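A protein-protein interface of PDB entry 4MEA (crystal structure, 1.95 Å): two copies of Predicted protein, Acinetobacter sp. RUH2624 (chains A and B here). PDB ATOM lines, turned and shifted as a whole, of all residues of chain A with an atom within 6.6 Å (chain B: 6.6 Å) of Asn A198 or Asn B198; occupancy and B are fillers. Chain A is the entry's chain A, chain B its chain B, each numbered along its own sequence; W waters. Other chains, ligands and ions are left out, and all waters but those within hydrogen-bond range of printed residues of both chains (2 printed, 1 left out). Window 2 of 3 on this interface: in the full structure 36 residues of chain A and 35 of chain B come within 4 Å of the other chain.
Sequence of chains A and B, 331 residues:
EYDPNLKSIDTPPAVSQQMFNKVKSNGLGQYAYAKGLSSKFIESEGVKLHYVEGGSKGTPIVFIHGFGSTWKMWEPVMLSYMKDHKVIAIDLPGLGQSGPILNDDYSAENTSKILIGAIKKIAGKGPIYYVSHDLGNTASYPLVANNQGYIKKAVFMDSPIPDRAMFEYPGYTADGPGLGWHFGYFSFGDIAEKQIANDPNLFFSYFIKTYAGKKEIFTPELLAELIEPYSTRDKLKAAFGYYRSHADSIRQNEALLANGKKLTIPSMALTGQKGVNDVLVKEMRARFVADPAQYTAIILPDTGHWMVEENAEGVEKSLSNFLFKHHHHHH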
ATOM      1  N   PRO A  13     -20.441 -27.606   1.126  1.00  0.00           N
ATOM      2  CA  PRO A  13     -21.473 -28.606   0.818  1.00  0.00           C
ATOM      3  C   PRO A  13     -21.636 -29.665   1.929  1.00  0.00           C
ATOM      4  O   PRO A  13     -22.750 -30.127   2.180  1.00  0.00           O
ATOM      5  CB  PRO A  13     -20.944 -29.254  -0.463  1.00  0.00           C
ATOM      6  CG  PRO A  13     -20.164 -28.157  -1.146  1.00  0.00           C
ATOM      7  CD  PRO A  13     -19.593 -27.291  -0.042  1.00  0.00           C
ATOM      8  N   ALA A 192     -28.237 -29.362 -15.039  1.00  0.00           N
ATOM      9  CA  ALA A 192     -28.786 -28.746 -13.831  1.00  0.00           C
ATOM     10  C   ALA A 192     -28.813 -29.783 -12.710  1.00  0.00           C
ATOM     11  O   ALA A 192     -28.385 -29.520 -11.589  1.00  0.00           O
ATOM     12  CB  ALA A 192     -30.185 -28.194 -14.078  1.00  0.00           C
ATOM     13  N   GLU A 193     -29.315 -30.968 -13.023  1.00  0.00           N
ATOM     14  CA  GLU A 193     -29.351 -32.041 -12.030  1.00  0.00           C
ATOM     15  C   GLU A 193     -27.974 -32.268 -11.402  1.00  0.00           C
ATOM     16  O   GLU A 193     -27.831 -32.282 -10.176  1.00  0.00           O
ATOM     17  CB  GLU A 193     -29.846 -33.342 -12.659  1.00  0.00           C
ATOM     18  CG  GLU A 193     -29.650 -34.553 -11.745  1.00  0.00           C
ATOM     19  CD  GLU A 193     -29.891 -35.862 -12.460  1.00  0.00           C
ATOM     20  OE1 GLU A 193     -30.542 -35.850 -13.535  1.00  0.00           O
ATOM     21  OE2 GLU A 193     -29.421 -36.901 -11.946  1.00  0.00           O
ATOM     22  N   LYS A 194     -26.965 -32.448 -12.249  1.00  0.00           N
ATOM     23  CA  LYS A 194     -25.607 -32.730 -11.783  1.00  0.00           C
ATOM     24  C   LYS A 194     -24.964 -31.552 -11.039  1.00  0.00           C
ATOM     25  O   LYS A 194     -24.342 -31.736  -9.982  1.00  0.00           O
ATOM     26  CB  LYS A 194     -24.723 -33.176 -12.952  1.00  0.00           C
ATOM     27  CG  LYS A 194     -24.969 -34.615 -13.428  1.00  0.00           C
ATOM     28  CD  LYS A 194     -23.977 -34.971 -14.528  1.00  0.00           C
ATOM     29  CE  LYS A 194     -24.016 -36.440 -14.890  1.00  0.00           C
ATOM     30  NZ  LYS A 194     -22.985 -36.732 -15.902  1.00  0.00           N
ATOM     31  N   GLN A 195     -25.104 -30.344 -11.583  1.00  0.00           N
ATOM     32  CA  GLN A 195     -24.479 -29.182 -10.957  1.00  0.00           C
ATOM     33  C   GLN A 195     -25.127 -28.862  -9.614  1.00  0.00           C
ATOM     34  O   GLN A 195     -24.440 -28.573  -8.631  1.00  0.00           O
ATOM     35  CB  GLN A 195     -24.540 -27.963 -11.874  1.00  0.00           C
ATOM     36  CG  GLN A 195     -23.610 -28.065 -13.080  1.00  0.00           C
ATOM     37  CD  GLN A 195     -23.539 -26.779 -13.863  1.00  0.00           C
ATOM     38  OE1 GLN A 195     -24.542 -26.097 -14.050  1.00  0.00           O
ATOM     39  NE2 GLN A 195     -22.348 -26.434 -14.316  1.00  0.00           N
ATOM     40  N   ILE A 196     -26.454 -28.903  -9.583  1.00  0.00           N
ATOM     41  CA  ILE A 196     -27.185 -28.569  -8.367  1.00  0.00           C
ATOM     42  C   ILE A 196     -26.989 -29.640  -7.291  1.00  0.00           C
ATOM     43  O   ILE A 196     -26.851 -29.312  -6.108  1.00  0.00           O
ATOM     44  CB  ILE A 196     -28.673 -28.277  -8.659  1.00  0.00           C
ATOM     45  CG1 ILE A 196     -28.782 -26.990  -9.495  1.00  0.00           C
ATOM     46  CG2 ILE A 196     -29.450 -28.114  -7.359  1.00  0.00           C
ATOM     47  CD1 ILE A 196     -30.174 -26.704 -10.070  1.00  0.00           C
ATOM     48  N   ALA A 197     -26.940 -30.913  -7.688  1.00  0.00           N
ATOM     49  CA  ALA A 197     -26.704 -31.980  -6.712  1.00  0.00           C
ATOM     50  C   ALA A 197     -25.378 -31.788  -5.982  1.00  0.00           C
ATOM     51  O   ALA A 197     -25.229 -32.208  -4.831  1.00  0.00           O
ATOM     52  CB  ALA A 197     -26.753 -33.378  -7.377  1.00  0.00           C
ATOM     53  N   ASN A 198     -24.408 -31.164  -6.646  1.00  0.00           N
ATOM     54  CA  ASN A 198     -23.117 -30.924  -6.002  1.00  0.00           C
ATOM     55  C   ASN A 198     -23.206 -29.963  -4.818  1.00  0.00           C
ATOM     56  O   ASN A 198     -22.450 -30.081  -3.848  1.00  0.00           O
ATOM     57  CB  ASN A 198     -22.060 -30.440  -7.006  1.00  0.00           C
ATOM     58  CG  ASN A 198     -20.742 -30.080  -6.328  1.00  0.00           C
ATOM     59  OD1 ASN A 198     -20.483 -28.913  -6.012  1.00  0.00           O
ATOM     60  ND2 ASN A 198     -19.909 -31.090  -6.088  1.00  0.00           N
ATOM     61  N   ASP A 199     -24.118 -29.001  -4.899  1.00  0.00           N
ATOM     62  CA  ASP A 199     -24.303 -28.048  -3.802  1.00  0.00           C
ATOM     63  C   ASP A 199     -25.708 -27.463  -3.869  1.00  0.00           C
ATOM     64  O   ASP A 199     -25.896 -26.354  -4.360  1.00  0.00           O
ATOM     65  CB  ASP A 199     -23.256 -26.931  -3.879  1.00  0.00           C
ATOM     66  CG  ASP A 199     -23.159 -26.123  -2.593  1.00  0.00           C
ATOM     67  OD1 ASP A 199     -24.098 -26.173  -1.773  1.00  0.00           O
ATOM     68  OD2 ASP A 199     -22.139 -25.421  -2.411  1.00  0.00           O
ATOM     69  N   PRO A 200     -26.710 -28.227  -3.399  1.00  0.00           N
ATOM     70  CA  PRO A 200     -28.104 -27.767  -3.486  1.00  0.00           C
ATOM     71  C   PRO A 200     -28.346 -26.518  -2.645  1.00  0.00           C
ATOM     72  O   PRO A 200     -29.110 -25.651  -3.056  1.00  0.00           O
ATOM     73  CB  PRO A 200     -28.908 -28.949  -2.923  1.00  0.00           C
ATOM     74  CG  PRO A 200     -28.000 -30.146  -3.079  1.00  0.00           C
ATOM     75  CD  PRO A 200     -26.605 -29.605  -2.884  1.00  0.00           C
ATOM     76  N   LEU A 202     -26.342 -24.034  -2.068  1.00  0.00           N
ATOM     77  CA  LEU A 202     -25.835 -22.879  -2.807  1.00  0.00           C
ATOM     78  C   LEU A 202     -26.837 -22.422  -3.857  1.00  0.00           C
ATOM     79  O   LEU A 202     -27.222 -21.245  -3.894  1.00  0.00           O
ATOM     80  CB  LEU A 202     -24.486 -23.210  -3.474  1.00  0.00           C
ATOM     81  CG  LEU A 202     -23.917 -22.211  -4.489  1.00  0.00           C
ATOM     82  CD1 LEU A 202     -23.624 -20.872  -3.816  1.00  0.00           C
ATOM     83  CD2 LEU A 202     -22.647 -22.769  -5.143  1.00  0.00           C
ATOM     84  N   ARG A 233     -29.855 -36.330  -6.435  1.00  0.00           N
ATOM     85  CA  ARG A 233     -30.017 -36.424  -7.889  1.00  0.00           C
ATOM     86  C   ARG A 233     -31.394 -36.945  -8.298  1.00  0.00           C
ATOM     87  O   ARG A 233     -31.972 -36.485  -9.290  1.00  0.00           O
ATOM     88  CB  ARG A 233     -28.945 -37.326  -8.523  1.00  0.00           C
ATOM     89  CG  ARG A 233     -27.499 -36.972  -8.218  1.00  0.00           C
ATOM     90  CD  ARG A 233     -26.746 -36.402  -9.415  1.00  0.00           C
ATOM     91  NE  ARG A 233     -27.057 -37.005 -10.717  1.00  0.00           N
ATOM     92  CZ  ARG A 233     -26.224 -37.767 -11.430  1.00  0.00           C
ATOM     93  NH1 ARG A 233     -25.019 -38.067 -10.971  1.00  0.00           N
ATOM     94  NH2 ARG A 233     -26.596 -38.232 -12.615  1.00  0.00           N
ATOM     95  N   LEU A 236     -33.917 -34.138  -7.966  1.00  0.00           N
ATOM     96  CA  LEU A 236     -33.633 -33.126  -8.980  1.00  0.00           C
ATOM     97  C   LEU A 236     -33.967 -33.639 -10.370  1.00  0.00           C
ATOM     98  O   LEU A 236     -34.531 -32.911 -11.184  1.00  0.00           O
ATOM     99  CB  LEU A 236     -32.169 -32.691  -8.912  1.00  0.00           C
ATOM    100  CG  LEU A 236     -31.833 -31.901  -7.646  1.00  0.00           C
ATOM    101  CD1 LEU A 236     -30.330 -31.783  -7.477  1.00  0.00           C
ATOM    102  CD2 LEU A 236     -32.500 -30.512  -7.684  1.00  0.00           C
ATOM    103  N   PRO B  13     -13.971 -34.781 -11.330  1.00  0.00           N
ATOM    104  CA  PRO B  13     -13.342 -33.455 -11.444  1.00  0.00           C
ATOM    105  C   PRO B  13     -11.853 -33.502 -11.132  1.00  0.00           C
ATOM    106  O   PRO B  13     -11.091 -32.723 -11.695  1.00  0.00           O
ATOM    107  CB  PRO B  13     -14.090 -32.625 -10.398  1.00  0.00           C
ATOM    108  CG  PRO B  13     -15.451 -33.275 -10.322  1.00  0.00           C
ATOM    109  CD  PRO B  13     -15.205 -34.749 -10.522  1.00  0.00           C
ATOM    110  N   ALA B 192     -23.279 -19.436 -11.881  1.00  0.00           N
ATOM    111  CA  ALA B 192     -22.583 -20.156 -12.948  1.00  0.00           C
ATOM    112  C   ALA B 192     -21.076 -20.254 -12.678  1.00  0.00           C
ATOM    113  O   ALA B 192     -20.470 -21.312 -12.867  1.00  0.00           O
ATOM    114  CB  ALA B 192     -22.854 -19.520 -14.329  1.00  0.00           C
ATOM    115  N   GLU B 193     -20.469 -19.150 -12.251  1.00  0.00           N
ATOM    116  CA  GLU B 193     -19.051 -19.164 -11.901  1.00  0.00           C
ATOM    117  C   GLU B 193     -18.771 -20.288 -10.889  1.00  0.00           C
ATOM    118  O   GLU B 193     -17.860 -21.107 -11.062  1.00  0.00           O
ATOM    119  CB  GLU B 193     -18.626 -17.814 -11.310  1.00  0.00           C
ATOM    120  CG  GLU B 193     -17.291 -17.884 -10.557  1.00  0.00           C
ATOM    121  CD  GLU B 193     -16.993 -16.641  -9.735  1.00  0.00           C
ATOM    122  OE1 GLU B 193     -17.541 -15.562 -10.044  1.00  0.00           O
ATOM    123  OE2 GLU B 193     -16.213 -16.748  -8.765  1.00  0.00           O
ATOM    124  N   LYS B 194     -19.572 -20.334  -9.833  1.00  0.00           N
ATOM    125  CA  LYS B 194     -19.349 -21.298  -8.768  1.00  0.00           C
ATOM    126  C   LYS B 194     -19.637 -22.747  -9.175  1.00  0.00           C
ATOM    127  O   LYS B 194     -18.858 -23.651  -8.874  1.00  0.00           O
ATOM    128  CB  LYS B 194     -20.158 -20.918  -7.534  1.00  0.00           C
ATOM    129  CG  LYS B 194     -19.465 -19.874  -6.656  1.00  0.00           C
ATOM    130  CD  LYS B 194     -20.286 -19.596  -5.408  1.00  0.00           C
ATOM    131  CE  LYS B 194     -19.543 -18.664  -4.457  1.00  0.00           C
ATOM    132  NZ  LYS B 194     -20.342 -18.433  -3.214  1.00  0.00           N
ATOM    133  N   GLN B 195     -20.756 -22.965  -9.849  1.00  0.00           N
ATOM    134  CA  GLN B 195     -21.150 -24.318 -10.231  1.00  0.00           C
ATOM    135  C   GLN B 195     -20.201 -24.880 -11.273  1.00  0.00           C
ATOM    136  O   GLN B 195     -19.778 -26.032 -11.183  1.00  0.00           O
ATOM    137  CB  GLN B 195     -22.591 -24.339 -10.743  1.00  0.00           C
ATOM    138  CG  GLN B 195     -23.619 -24.056  -9.643  1.00  0.00           C
ATOM    139  CD  GLN B 195     -25.033 -24.375 -10.070  1.00  0.00           C
ATOM    140  OE1 GLN B 195     -25.796 -24.981  -9.318  1.00  0.00           O
ATOM    141  NE2 GLN B 195     -25.389 -23.969 -11.276  1.00  0.00           N
ATOM    142  N   ILE B 196     -19.851 -24.056 -12.256  1.00  0.00           N
ATOM    143  CA  ILE B 196     -18.961 -24.506 -13.315  1.00  0.00           C
ATOM    144  C   ILE B 196     -17.542 -24.704 -12.787  1.00  0.00           C
ATOM    145  O   ILE B 196     -16.849 -25.629 -13.197  1.00  0.00           O
ATOM    146  CB  ILE B 196     -19.015 -23.555 -14.521  1.00  0.00           C
ATOM    147  CG1 ILE B 196     -20.432 -23.583 -15.112  1.00  0.00           C
ATOM    148  CG2 ILE B 196     -17.983 -23.945 -15.563  1.00  0.00           C
ATOM    149  CD1 ILE B 196     -20.695 -22.506 -16.143  1.00  0.00           C
ATOM    150  N   ALA B 197     -17.122 -23.860 -11.847  1.00  0.00           N
ATOM    151  CA  ALA B 197     -15.805 -24.028 -11.246  1.00  0.00           C
ATOM    152  C   ALA B 197     -15.682 -25.383 -10.536  1.00  0.00           C
ATOM    153  O   ALA B 197     -14.593 -25.949 -10.449  1.00  0.00           O
ATOM    154  CB  ALA B 197     -15.500 -22.891 -10.285  1.00  0.00           C
ATOM    155  N   ASN B 198     -16.790 -25.909 -10.028  1.00  0.00           N
ATOM    156  CA  ASN B 198     -16.744 -27.225  -9.375  1.00  0.00           C
ATOM    157  C   ASN B 198     -16.388 -28.340 -10.356  1.00  0.00           C
ATOM    158  O   ASN B 198     -15.707 -29.288  -9.996  1.00  0.00           O
ATOM    159  CB  ASN B 198     -18.057 -27.554  -8.659  1.00  0.00           C
ATOM    160  CG  ASN B 198     -18.034 -28.937  -8.005  1.00  0.00           C
ATOM    161  OD1 ASN B 198     -18.645 -29.892  -8.503  1.00  0.00           O
ATOM    162  ND2 ASN B 198     -17.311 -29.052  -6.897  1.00  0.00           N
ATOM    163  N   ASP B 199     -16.831 -28.214 -11.602  1.00  0.00           N
ATOM    164  CA  ASP B 199     -16.540 -29.227 -12.616  1.00  0.00           C
ATOM    165  C   ASP B 199     -16.620 -28.605 -14.015  1.00  0.00           C
ATOM    166  O   ASP B 199     -17.633 -28.746 -14.697  1.00  0.00           O
ATOM    167  CB  ASP B 199     -17.537 -30.379 -12.477  1.00  0.00           C
ATOM    168  CG  ASP B 199     -17.137 -31.608 -13.263  1.00  0.00           C
ATOM    169  OD1 ASP B 199     -16.234 -31.505 -14.126  1.00  0.00           O
ATOM    170  OD2 ASP B 199     -17.747 -32.680 -13.028  1.00  0.00           O
ATOM    171  N   PRO B 200     -15.564 -27.879 -14.430  1.00  0.00           N
ATOM    172  CA  PRO B 200     -15.577 -27.201 -15.736  1.00  0.00           C
ATOM    173  C   PRO B 200     -15.667 -28.192 -16.886  1.00  0.00           C
ATOM    174  O   PRO B 200     -16.367 -27.936 -17.864  1.00  0.00           O
ATOM    175  CB  PRO B 200     -14.221 -26.462 -15.782  1.00  0.00           C
ATOM    176  CG  PRO B 200     -13.752 -26.399 -14.381  1.00  0.00           C
ATOM    177  CD  PRO B 200     -14.351 -27.575 -13.651  1.00  0.00           C
ATOM    178  N   ARG B 233     -12.139 -20.028 -10.900  1.00  0.00           N
ATOM    179  CA  ARG B 233     -13.192 -19.060 -10.555  1.00  0.00           C
ATOM    180  C   ARG B 233     -12.893 -17.686 -11.128  1.00  0.00           C
ATOM    181  O   ARG B 233     -13.805 -16.976 -11.545  1.00  0.00           O
ATOM    182  CB  ARG B 233     -13.378 -18.913  -9.033  1.00  0.00           C
ATOM    183  CG  ARG B 233     -13.704 -20.193  -8.261  1.00  0.00           C
ATOM    184  CD  ARG B 233     -15.146 -20.270  -7.776  1.00  0.00           C
ATOM    185  NE  ARG B 233     -15.720 -18.987  -7.364  1.00  0.00           N
ATOM    186  CZ  ARG B 233     -15.940 -18.605  -6.108  1.00  0.00           C
ATOM    187  NH1 ARG B 233     -15.631 -19.397  -5.089  1.00  0.00           N
ATOM    188  NH2 ARG B 233     -16.479 -17.416  -5.872  1.00  0.00           N
ATOM    189  N   LEU B 236     -13.743 -17.662 -14.929  1.00  0.00           N
ATOM    190  CA  LEU B 236     -15.193 -17.741 -15.107  1.00  0.00           C
ATOM    191  C   LEU B 236     -15.907 -16.460 -14.650  1.00  0.00           C
ATOM    192  O   LEU B 236     -16.855 -16.020 -15.289  1.00  0.00           O
ATOM    193  CB  LEU B 236     -15.770 -18.968 -14.392  1.00  0.00           C
ATOM    194  CG  LEU B 236     -15.328 -20.327 -14.929  1.00  0.00           C
ATOM    195  CD1 LEU B 236     -15.474 -21.395 -13.842  1.00  0.00           C
ATOM    196  CD2 LEU B 236     -16.108 -20.709 -16.207  1.00  0.00           C
HETATM  197  O   HOH W   1     -20.290 -28.070 -13.685  1.00  0.00           O
HETATM  198  O   HOH W   2     -21.983 -27.536  -9.433  1.00  0.00           O
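ND2 of Asn A198 is in hydrogen-bond range of OD1 of Asn B198 (3.0 Å).
The backbone NH (N) of Leu A202 is in hydrogen-bond range of the side-chain carboxylate (OD1) of Asp A199 (3.1 Å).
Among the printed residues, pairs that only touch across the chains: Gln A195 with Gln B195 (3.6 Å), Gln A195 with Ile B196 (3.5 Å), Ile A196 with Gln B195 (3.6 Å) and Leu A202 with Lys B194 (3.9 Å).
Of the printed residues of chain B, Gln A195 touches Gln B195 and Ile B196.
Printed residues of chain B within 4 Å of Ile A196: Gln B195 (3.6 Å).
Asn A198 touches one residue of chain B.
Pro A200 touches none of the printed residues of chain B.
Of the printed residues of chain B, Leu A202 touches Lys B194 (3.9 Å).
Printed residues of chain A within 4 Å of Gln B195: Gln A195 (3.6 Å) and Ile A196 (3.6 Å).
Printed residues of chain A within 4 Å of Ile B196: Gln A195.
Printed residues of chain A within 4 Å of Asn B198: Asn A198.
Leu B236 touches none of the printed residues of chain A.
The nearest residue of chain B that does not touch Asn A198 is Gln B195 (6.0 Å).
The nearest residue of chain A that does not touch Asn B198 is Gln A195 (5.9 Å).
Of the 12 printed residues of chain B, 4 touch a printed residue of chain A.
Of the 13 printed residues of chain A, 4 touch a printed residue of chain B.
Hydrophobic or aromatic side chains of chain A that line the printed part of chain B: Ile A196 and Leu A202.
Among the printed residues, 5 pairs touch across the chains.
Gln B195 touches its own counterpart, Gln A195.
Gln A195 touches Ile B196, and with the chains exchanged Ile A196 touches Gln B195.
Asn A198 touches its own counterpart, Asn B198.
Of the 5 pairs that touch across the chains among the printed residues, 4 have their exchanged pair printed and touching as well.
Water W1 lies within hydrogen-bond range of NE2 of Gln A195, O of Asp B199 and O of Gln B195.
Water W2 bridges the backbone carbonyl oxygen of Gln A195 and the backbone carbonyl oxygen of Gln B195.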
